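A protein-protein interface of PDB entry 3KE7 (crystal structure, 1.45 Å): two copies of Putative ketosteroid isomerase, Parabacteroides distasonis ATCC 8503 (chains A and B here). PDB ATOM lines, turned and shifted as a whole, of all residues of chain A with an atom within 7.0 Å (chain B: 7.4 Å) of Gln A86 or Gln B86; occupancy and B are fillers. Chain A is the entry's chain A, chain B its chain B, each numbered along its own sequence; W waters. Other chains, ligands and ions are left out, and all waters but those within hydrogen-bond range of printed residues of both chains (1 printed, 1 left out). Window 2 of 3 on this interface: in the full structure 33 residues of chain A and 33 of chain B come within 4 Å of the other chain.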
ATOM      1  N   ILE A  15      -3.453  17.296  15.970  1.00  0.00           N
ATOM      2  CA  ILE A  15      -4.474  18.210  16.457  1.00  0.00           C
ATOM      3  C   ILE A  15      -5.707  17.422  16.908  1.00  0.00           C
ATOM      4  O   ILE A  15      -6.184  17.650  18.029  1.00  0.00           O
ATOM      5  CB  ILE A  15      -4.759  19.348  15.459  1.00  0.00           C
ATOM      6  CG1 ILE A  15      -3.530  20.255  15.356  1.00  0.00           C
ATOM      7  CG2 ILE A  15      -6.015  20.106  15.867  1.00  0.00           C
ATOM      8  CD1 ILE A  15      -3.516  21.093  14.101  1.00  0.00           C
ATOM      9  N   VAL A  84     -10.489  19.553  10.987  1.00  0.00           N
ATOM     10  CA  VAL A  84      -9.543  20.649  11.117  1.00  0.00           C
ATOM     11  C   VAL A  84      -9.544  21.455   9.850  1.00  0.00           C
ATOM     12  O   VAL A  84      -9.480  20.911   8.752  1.00  0.00           O
ATOM     13  CB  VAL A  84      -8.117  20.107  11.453  1.00  0.00           C
ATOM     14  CG1 VAL A  84      -7.095  21.289  11.512  1.00  0.00           C
ATOM     15  CG2 VAL A  84      -8.121  19.357  12.764  1.00  0.00           C
ATOM     16  N   ALA A  85      -9.609  22.775   9.994  1.00  0.00           N
ATOM     17  CA  ALA A  85      -9.620  23.725   8.885  1.00  0.00           C
ATOM     18  C   ALA A  85      -8.843  24.936   9.318  1.00  0.00           C
ATOM     19  O   ALA A  85      -9.377  25.799  10.041  1.00  0.00           O
ATOM     20  CB  ALA A  85     -11.048  24.156   8.589  1.00  0.00           C
ATOM     21  N   GLN A  86      -7.619  24.996   8.877  1.00  0.00           N
ATOM     22  CA  GLN A  86      -6.696  26.100   9.201  1.00  0.00           C
ATOM     23  C   GLN A  86      -6.653  26.279  10.738  1.00  0.00           C
ATOM     24  O   GLN A  86      -6.218  25.303  11.484  1.00  0.00           O
ATOM     25  CB  GLN A  86      -7.061  27.387   8.452  1.00  0.00           C
ATOM     26  CG  GLN A  86      -7.057  27.270   6.906  1.00  0.00           C
ATOM     27  CD  GLN A  86      -5.682  27.000   6.345  1.00  0.00           C
ATOM     28  OE1 GLN A  86      -4.711  27.665   6.705  1.00  0.00           O
ATOM     29  NE2 GLN A  86      -5.593  26.029   5.433  1.00  0.00           N
ATOM     30  N   ASN A  87      -7.207  27.387  11.258  1.00  0.00           N
ATOM     31  CA  ASN A  87      -7.102  27.649  12.671  1.00  0.00           C
ATOM     32  C   ASN A  87      -8.339  27.247  13.454  1.00  0.00           C
ATOM     33  O   ASN A  87      -8.562  27.758  14.523  1.00  0.00           O
ATOM     34  CB  ASN A  87      -6.806  29.138  12.928  1.00  0.00           C
ATOM     35  CG  ASN A  87      -7.934  30.064  12.517  1.00  0.00           C
ATOM     36  OD1 ASN A  87      -8.787  29.741  11.658  1.00  0.00           O
ATOM     37  ND2 ASN A  87      -7.949  31.270  13.124  1.00  0.00           N
ATOM     38  N   ILE A  88      -9.103  26.298  12.939  1.00  0.00           N
ATOM     39  CA  ILE A  88     -10.337  25.812  13.580  1.00  0.00           C
ATOM     40  C   ILE A  88     -10.324  24.283  13.656  1.00  0.00           C
ATOM     41  O   ILE A  88      -9.900  23.587  12.729  1.00  0.00           O
ATOM     42  CB  ILE A  88     -11.554  26.256  12.776  1.00  0.00           C
ATOM     43  CG1 ILE A  88     -11.803  27.783  12.927  1.00  0.00           C
ATOM     44  CG2 ILE A  88     -12.825  25.418  13.123  1.00  0.00           C
ATOM     45  CD1 ILE A  88     -12.272  28.196  14.319  1.00  0.00           C
ATOM     46  N   ALA A  89     -10.749  23.775  14.790  1.00  0.00           N
ATOM     47  CA  ALA A  89     -10.992  22.355  14.959  1.00  0.00           C
ATOM     48  C   ALA A  89     -12.404  22.182  15.482  1.00  0.00           C
ATOM     49  O   ALA A  89     -12.753  22.703  16.513  1.00  0.00           O
ATOM     50  CB  ALA A  89      -9.968  21.676  15.930  1.00  0.00           C
ATOM     51  N   ARG A 114      -7.512  28.159  17.072  1.00  0.00           N
ATOM     52  CA  ARG A 114      -6.103  28.369  17.401  1.00  0.00           C
ATOM     53  C   ARG A 114      -5.860  29.862  17.274  1.00  0.00           C
ATOM     54  O   ARG A 114      -5.915  30.425  16.165  1.00  0.00           O
ATOM     55  CB  ARG A 114      -5.163  27.615  16.473  1.00  0.00           C
ATOM     56  CG  ARG A 114      -3.694  27.646  16.944  1.00  0.00           C
ATOM     57  CD  ARG A 114      -2.777  26.638  16.163  1.00  0.00           C
ATOM     58  NE  ARG A 114      -2.917  26.852  14.735  1.00  0.00           N
ATOM     59  CZ  ARG A 114      -2.690  25.949  13.793  1.00  0.00           C
ATOM     60  NH1 ARG A 114      -2.298  24.701  14.093  1.00  0.00           N
ATOM     61  NH2 ARG A 114      -2.867  26.307  12.522  1.00  0.00           N
ATOM     62  N   TRP A 120      -5.286  26.736  21.686  1.00  0.00           N
ATOM     63  CA  TRP A 120      -6.609  26.357  21.157  1.00  0.00           C
ATOM     64  C   TRP A 120      -7.643  26.624  22.254  1.00  0.00           C
ATOM     65  O   TRP A 120      -7.508  26.139  23.378  1.00  0.00           O
ATOM     66  CB  TRP A 120      -6.640  24.897  20.719  1.00  0.00           C
ATOM     67  CG  TRP A 120      -5.798  24.606  19.557  1.00  0.00           C
ATOM     68  CD1 TRP A 120      -4.429  24.385  19.566  1.00  0.00           C
ATOM     69  CD2 TRP A 120      -6.207  24.490  18.220  1.00  0.00           C
ATOM     70  NE1 TRP A 120      -3.982  24.136  18.295  1.00  0.00           N
ATOM     71  CE2 TRP A 120      -5.060  24.175  17.454  1.00  0.00           C
ATOM     72  CE3 TRP A 120      -7.450  24.633  17.556  1.00  0.00           C
ATOM     73  CZ2 TRP A 120      -5.120  23.966  16.115  1.00  0.00           C
ATOM     74  CZ3 TRP A 120      -7.478  24.439  16.234  1.00  0.00           C
ATOM     75  CH2 TRP A 120      -6.325  24.128  15.516  1.00  0.00           C
ATOM     76  N   ILE B  15     -19.311  38.478   5.100  1.00  0.00           N
ATOM     77  CA  ILE B  15     -19.449  37.028   5.340  1.00  0.00           C
ATOM     78  C   ILE B  15     -20.612  36.703   6.267  1.00  0.00           C
ATOM     79  O   ILE B  15     -21.396  35.829   5.954  1.00  0.00           O
ATOM     80  CB  ILE B  15     -18.109  36.384   5.830  1.00  0.00           C
ATOM     81  CG1 ILE B  15     -17.123  36.360   4.685  1.00  0.00           C
ATOM     82  CG2 ILE B  15     -18.343  34.965   6.338  1.00  0.00           C
ATOM     83  CD1 ILE B  15     -15.649  36.074   5.119  1.00  0.00           C
ATOM     84  N   GLN B  83     -19.322  33.766  13.673  1.00  0.00           N
ATOM     85  CA  GLN B  83     -17.930  33.879  14.042  1.00  0.00           C
ATOM     86  C   GLN B  83     -17.077  33.433  12.848  1.00  0.00           C
ATOM     87  O   GLN B  83     -17.218  32.281  12.368  1.00  0.00           O
ATOM     88  CB  GLN B  83     -17.647  32.984  15.244  1.00  0.00           C
ATOM     89  CG  GLN B  83     -18.381  33.328  16.502  1.00  0.00           C
ATOM     90  CD  GLN B  83     -18.422  32.142  17.472  1.00  0.00           C
ATOM     91  OE1 GLN B  83     -19.018  31.110  17.189  1.00  0.00           O
ATOM     92  NE2 GLN B  83     -17.790  32.305  18.622  1.00  0.00           N
ATOM     93  N   VAL B  84     -16.207  34.324  12.368  1.00  0.00           N
ATOM     94  CA  VAL B  84     -15.434  34.052  11.183  1.00  0.00           C
ATOM     95  C   VAL B  84     -13.976  33.833  11.544  1.00  0.00           C
ATOM     96  O   VAL B  84     -13.370  34.656  12.306  1.00  0.00           O
ATOM     97  CB  VAL B  84     -15.589  35.194  10.177  1.00  0.00           C
ATOM     98  CG1 VAL B  84     -14.832  34.903   8.854  1.00  0.00           C
ATOM     99  CG2 VAL B  84     -17.092  35.404   9.810  1.00  0.00           C
ATOM    100  N   ALA B  85     -13.421  32.742  11.036  1.00  0.00           N
ATOM    101  CA  ALA B  85     -12.018  32.350  11.277  1.00  0.00           C
ATOM    102  C   ALA B  85     -11.472  31.799  10.011  1.00  0.00           C
ATOM    103  O   ALA B  85     -11.660  30.604   9.690  1.00  0.00           O
ATOM    104  CB  ALA B  85     -11.919  31.307  12.353  1.00  0.00           C
ATOM    105  N   GLN B  86     -10.855  32.657   9.264  1.00  0.00           N
ATOM    106  CA  GLN B  86     -10.187  32.299   8.038  1.00  0.00           C
ATOM    107  C   GLN B  86     -11.224  31.651   7.092  1.00  0.00           C
ATOM    108  O   GLN B  86     -12.233  32.332   6.704  1.00  0.00           O
ATOM    109  CB  GLN B  86      -8.915  31.434   8.336  1.00  0.00           C
ATOM    110  CG  GLN B  86      -7.848  32.208   9.203  1.00  0.00           C
ATOM    111  CD  GLN B  86      -6.610  31.390   9.593  1.00  0.00           C
ATOM    112  OE1 GLN B  86      -6.375  30.316   9.076  1.00  0.00           O
ATOM    113  NE2 GLN B  86      -5.802  31.934  10.502  1.00  0.00           N
ATOM    114  N   ASN B  87     -11.084  30.347   6.827  1.00  0.00           N
ATOM    115  CA  ASN B  87     -11.982  29.667   5.910  1.00  0.00           C
ATOM    116  C   ASN B  87     -13.203  28.999   6.592  1.00  0.00           C
ATOM    117  O   ASN B  87     -13.851  28.157   5.985  1.00  0.00           O
ATOM    118  CB  ASN B  87     -11.214  28.634   5.080  1.00  0.00           C
ATOM    119  CG  ASN B  87     -10.715  27.428   5.886  1.00  0.00           C
ATOM    120  OD1 ASN B  87     -10.533  27.470   7.111  1.00  0.00           O
ATOM    121  ND2 ASN B  87     -10.497  26.297   5.153  1.00  0.00           N
ATOM    122  N   ILE B  88     -13.487  29.385   7.834  1.00  0.00           N
ATOM    123  CA  ILE B  88     -14.616  28.837   8.603  1.00  0.00           C
ATOM    124  C   ILE B  88     -15.536  29.974   9.066  1.00  0.00           C
ATOM    125  O   ILE B  88     -15.085  31.081   9.449  1.00  0.00           O
ATOM    126  CB  ILE B  88     -14.114  28.110   9.839  1.00  0.00           C
ATOM    127  CG1 ILE B  88     -13.440  26.796   9.422  1.00  0.00           C
ATOM    128  CG2 ILE B  88     -15.242  27.833  10.840  1.00  0.00           C
ATOM    129  CD1 ILE B  88     -14.394  25.699   8.962  1.00  0.00           C
ATOM    130  N   ALA B  89     -16.842  29.712   8.989  1.00  0.00           N
ATOM    131  CA  ALA B  89     -17.830  30.594   9.597  1.00  0.00           C
ATOM    132  C   ALA B  89     -18.700  29.737  10.480  1.00  0.00           C
ATOM    133  O   ALA B  89     -19.284  28.752  10.010  1.00  0.00           O
ATOM    134  CB  ALA B  89     -18.690  31.210   8.548  1.00  0.00           C
ATOM    135  N   TYR B 112     -19.791  26.368   8.521  1.00  0.00           N
ATOM    136  CA  TYR B 112     -19.563  26.473   7.094  1.00  0.00           C
ATOM    137  C   TYR B 112     -18.071  26.625   6.825  1.00  0.00           C
ATOM    138  O   TYR B 112     -17.348  27.281   7.605  1.00  0.00           O
ATOM    139  CB  TYR B 112     -20.248  27.731   6.518  1.00  0.00           C
ATOM    140  CG  TYR B 112     -21.757  27.685   6.338  1.00  0.00           C
ATOM    141  CD1 TYR B 112     -22.609  27.800   7.409  1.00  0.00           C
ATOM    142  CD2 TYR B 112     -22.309  27.593   5.069  1.00  0.00           C
ATOM    143  CE1 TYR B 112     -23.972  27.863   7.247  1.00  0.00           C
ATOM    144  CE2 TYR B 112     -23.675  27.605   4.885  1.00  0.00           C
ATOM    145  CZ  TYR B 112     -24.506  27.738   5.983  1.00  0.00           C
ATOM    146  OH  TYR B 112     -25.889  27.795   5.795  1.00  0.00           O
ATOM    147  N   ARG B 113     -17.603  25.993   5.759  1.00  0.00           N
ATOM    148  CA  ARG B 113     -16.235  26.044   5.337  1.00  0.00           C
ATOM    149  C   ARG B 113     -16.185  26.525   3.913  1.00  0.00           C
ATOM    150  O   ARG B 113     -16.939  26.025   3.074  1.00  0.00           O
ATOM    151  CB  ARG B 113     -15.556  24.659   5.453  1.00  0.00           C
ATOM    152  CG  ARG B 113     -14.060  24.631   4.981  1.00  0.00           C
ATOM    153  CD  ARG B 113     -13.407  23.264   5.133  1.00  0.00           C
ATOM    154  NE  ARG B 113     -14.137  22.296   4.344  1.00  0.00           N
ATOM    155  CZ  ARG B 113     -14.368  21.012   4.682  1.00  0.00           C
ATOM    156  NH1 ARG B 113     -13.900  20.480   5.817  1.00  0.00           N
ATOM    157  NH2 ARG B 113     -15.109  20.249   3.879  1.00  0.00           N
ATOM    158  N   ARG B 114     -15.305  27.484   3.650  1.00  0.00           N
ATOM    159  CA  ARG B 114     -15.138  28.019   2.320  1.00  0.00           C
ATOM    160  C   ARG B 114     -14.207  27.083   1.567  1.00  0.00           C
ATOM    161  O   ARG B 114     -13.083  26.857   2.012  1.00  0.00           O
ATOM    162  CB  ARG B 114     -14.556  29.436   2.387  1.00  0.00           C
ATOM    163  CG  ARG B 114     -14.469  30.107   0.981  1.00  0.00           C
ATOM    164  CD  ARG B 114     -13.994  31.552   1.094  1.00  0.00           C
ATOM    165  NE  ARG B 114     -12.702  31.577   1.748  1.00  0.00           N
ATOM    166  CZ  ARG B 114     -12.284  32.513   2.603  1.00  0.00           C
ATOM    167  NH1 ARG B 114     -13.046  33.577   2.909  1.00  0.00           N
ATOM    168  NH2 ARG B 114     -11.090  32.375   3.166  1.00  0.00           N
ATOM    169  N   TRP B 120     -19.186  28.318   0.085  1.00  0.00           N
ATOM    170  CA  TRP B 120     -19.303  27.997   1.507  1.00  0.00           C
ATOM    171  C   TRP B 120     -20.224  26.791   1.675  1.00  0.00           C
ATOM    172  O   TRP B 120     -21.383  26.814   1.192  1.00  0.00           O
ATOM    173  CB  TRP B 120     -19.877  29.154   2.270  1.00  0.00           C
ATOM    174  CG  TRP B 120     -18.967  30.292   2.314  1.00  0.00           C
ATOM    175  CD1 TRP B 120     -18.818  31.255   1.339  1.00  0.00           C
ATOM    176  CD2 TRP B 120     -18.029  30.630   3.353  1.00  0.00           C
ATOM    177  NE1 TRP B 120     -17.883  32.178   1.730  1.00  0.00           N
ATOM    178  CE2 TRP B 120     -17.388  31.826   2.960  1.00  0.00           C
ATOM    179  CE3 TRP B 120     -17.648  30.036   4.556  1.00  0.00           C
ATOM    180  CZ2 TRP B 120     -16.408  32.436   3.738  1.00  0.00           C
ATOM    181  CZ3 TRP B 120     -16.723  30.661   5.332  1.00  0.00           C
ATOM    182  CH2 TRP B 120     -16.090  31.839   4.920  1.00  0.00           C
HETATM  183  O   HOH W   1     -10.995  21.240   6.369  1.00  0.00           O
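The side-chain amide nitrogen of Asn A87 lies close to the side-chain amide nitrogen of Gln B86 (3.5 Å).
The backbone carbonyl oxygen (O) of Asn B87 sits at hydrogen-bond distance from the backbone NH (N) of Arg B114, at 2.8 Å.
O of Asn A87 is in hydrogen-bond range of N of Arg A114 (2.8 Å).
Among the printed residues, merely in contact across the chains: Gln A86 with Gln B86, Gln A86 with Asn B87, Ala A85 with Asn B87, Asn A87 with Ala B85, Ile A88 with Ala B85, Ala A85 with Ile B88 and Ile A88 with Ile B88.
Printed residues of chain B within 4 Å of Gln A86: Gln B86 (3.1 Å) and Asn B87 (3.5 Å).
Printed residues of chain A within 4 Å of Gln B86: Gln A86 (3.1 Å) and Asn A87 (3.4 Å).
Of the printed residues of chain B, Ala A85 touches Asn B87 and Ile B88.
Of the printed residues of chain B, Asn A87 touches Ala B85 and Gln B86.
Arg B113 touches none of the printed residues of chain A.
Gln B83 touches none of the printed residues of chain A.
The nearest printed residue of chain B that does not touch Gln A86 is Ala B85 (5.7 Å).
The nearest printed residue of chain A that does not touch Gln B86 is Ala A85 (5.5 Å).
Of the 9 printed residues of chain A, 4 touch a printed residue of chain B.
Hydrophobic or aromatic side chains of chain A that line the printed part of chain B: Ala A85 and Ile A88.
Of the 12 printed residues of chain B, 4 touch a printed residue of chain A.
Hydrophobic or aromatic side chains of chain B within 4 Å of the printed part of chain A: Ala B85 and Ile B88.
Ala A85 touches Asn B87, and with the chains exchanged Asn A87 touches Ala B85.
Ala A85 touches Ile B88, and with the chains exchanged Ile A88 touches Ala B85.
Gln A86 touches its own counterpart, Gln B86.
Gln A86 touches Asn B87, and with the chains exchanged Asn A87 touches Gln B86.
9 positions are printed for both chains.
Water W1 lies within hydrogen-bond range of O of Val A84 (2.8 Å) and NH1 of Arg B113 (3.1 Å).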
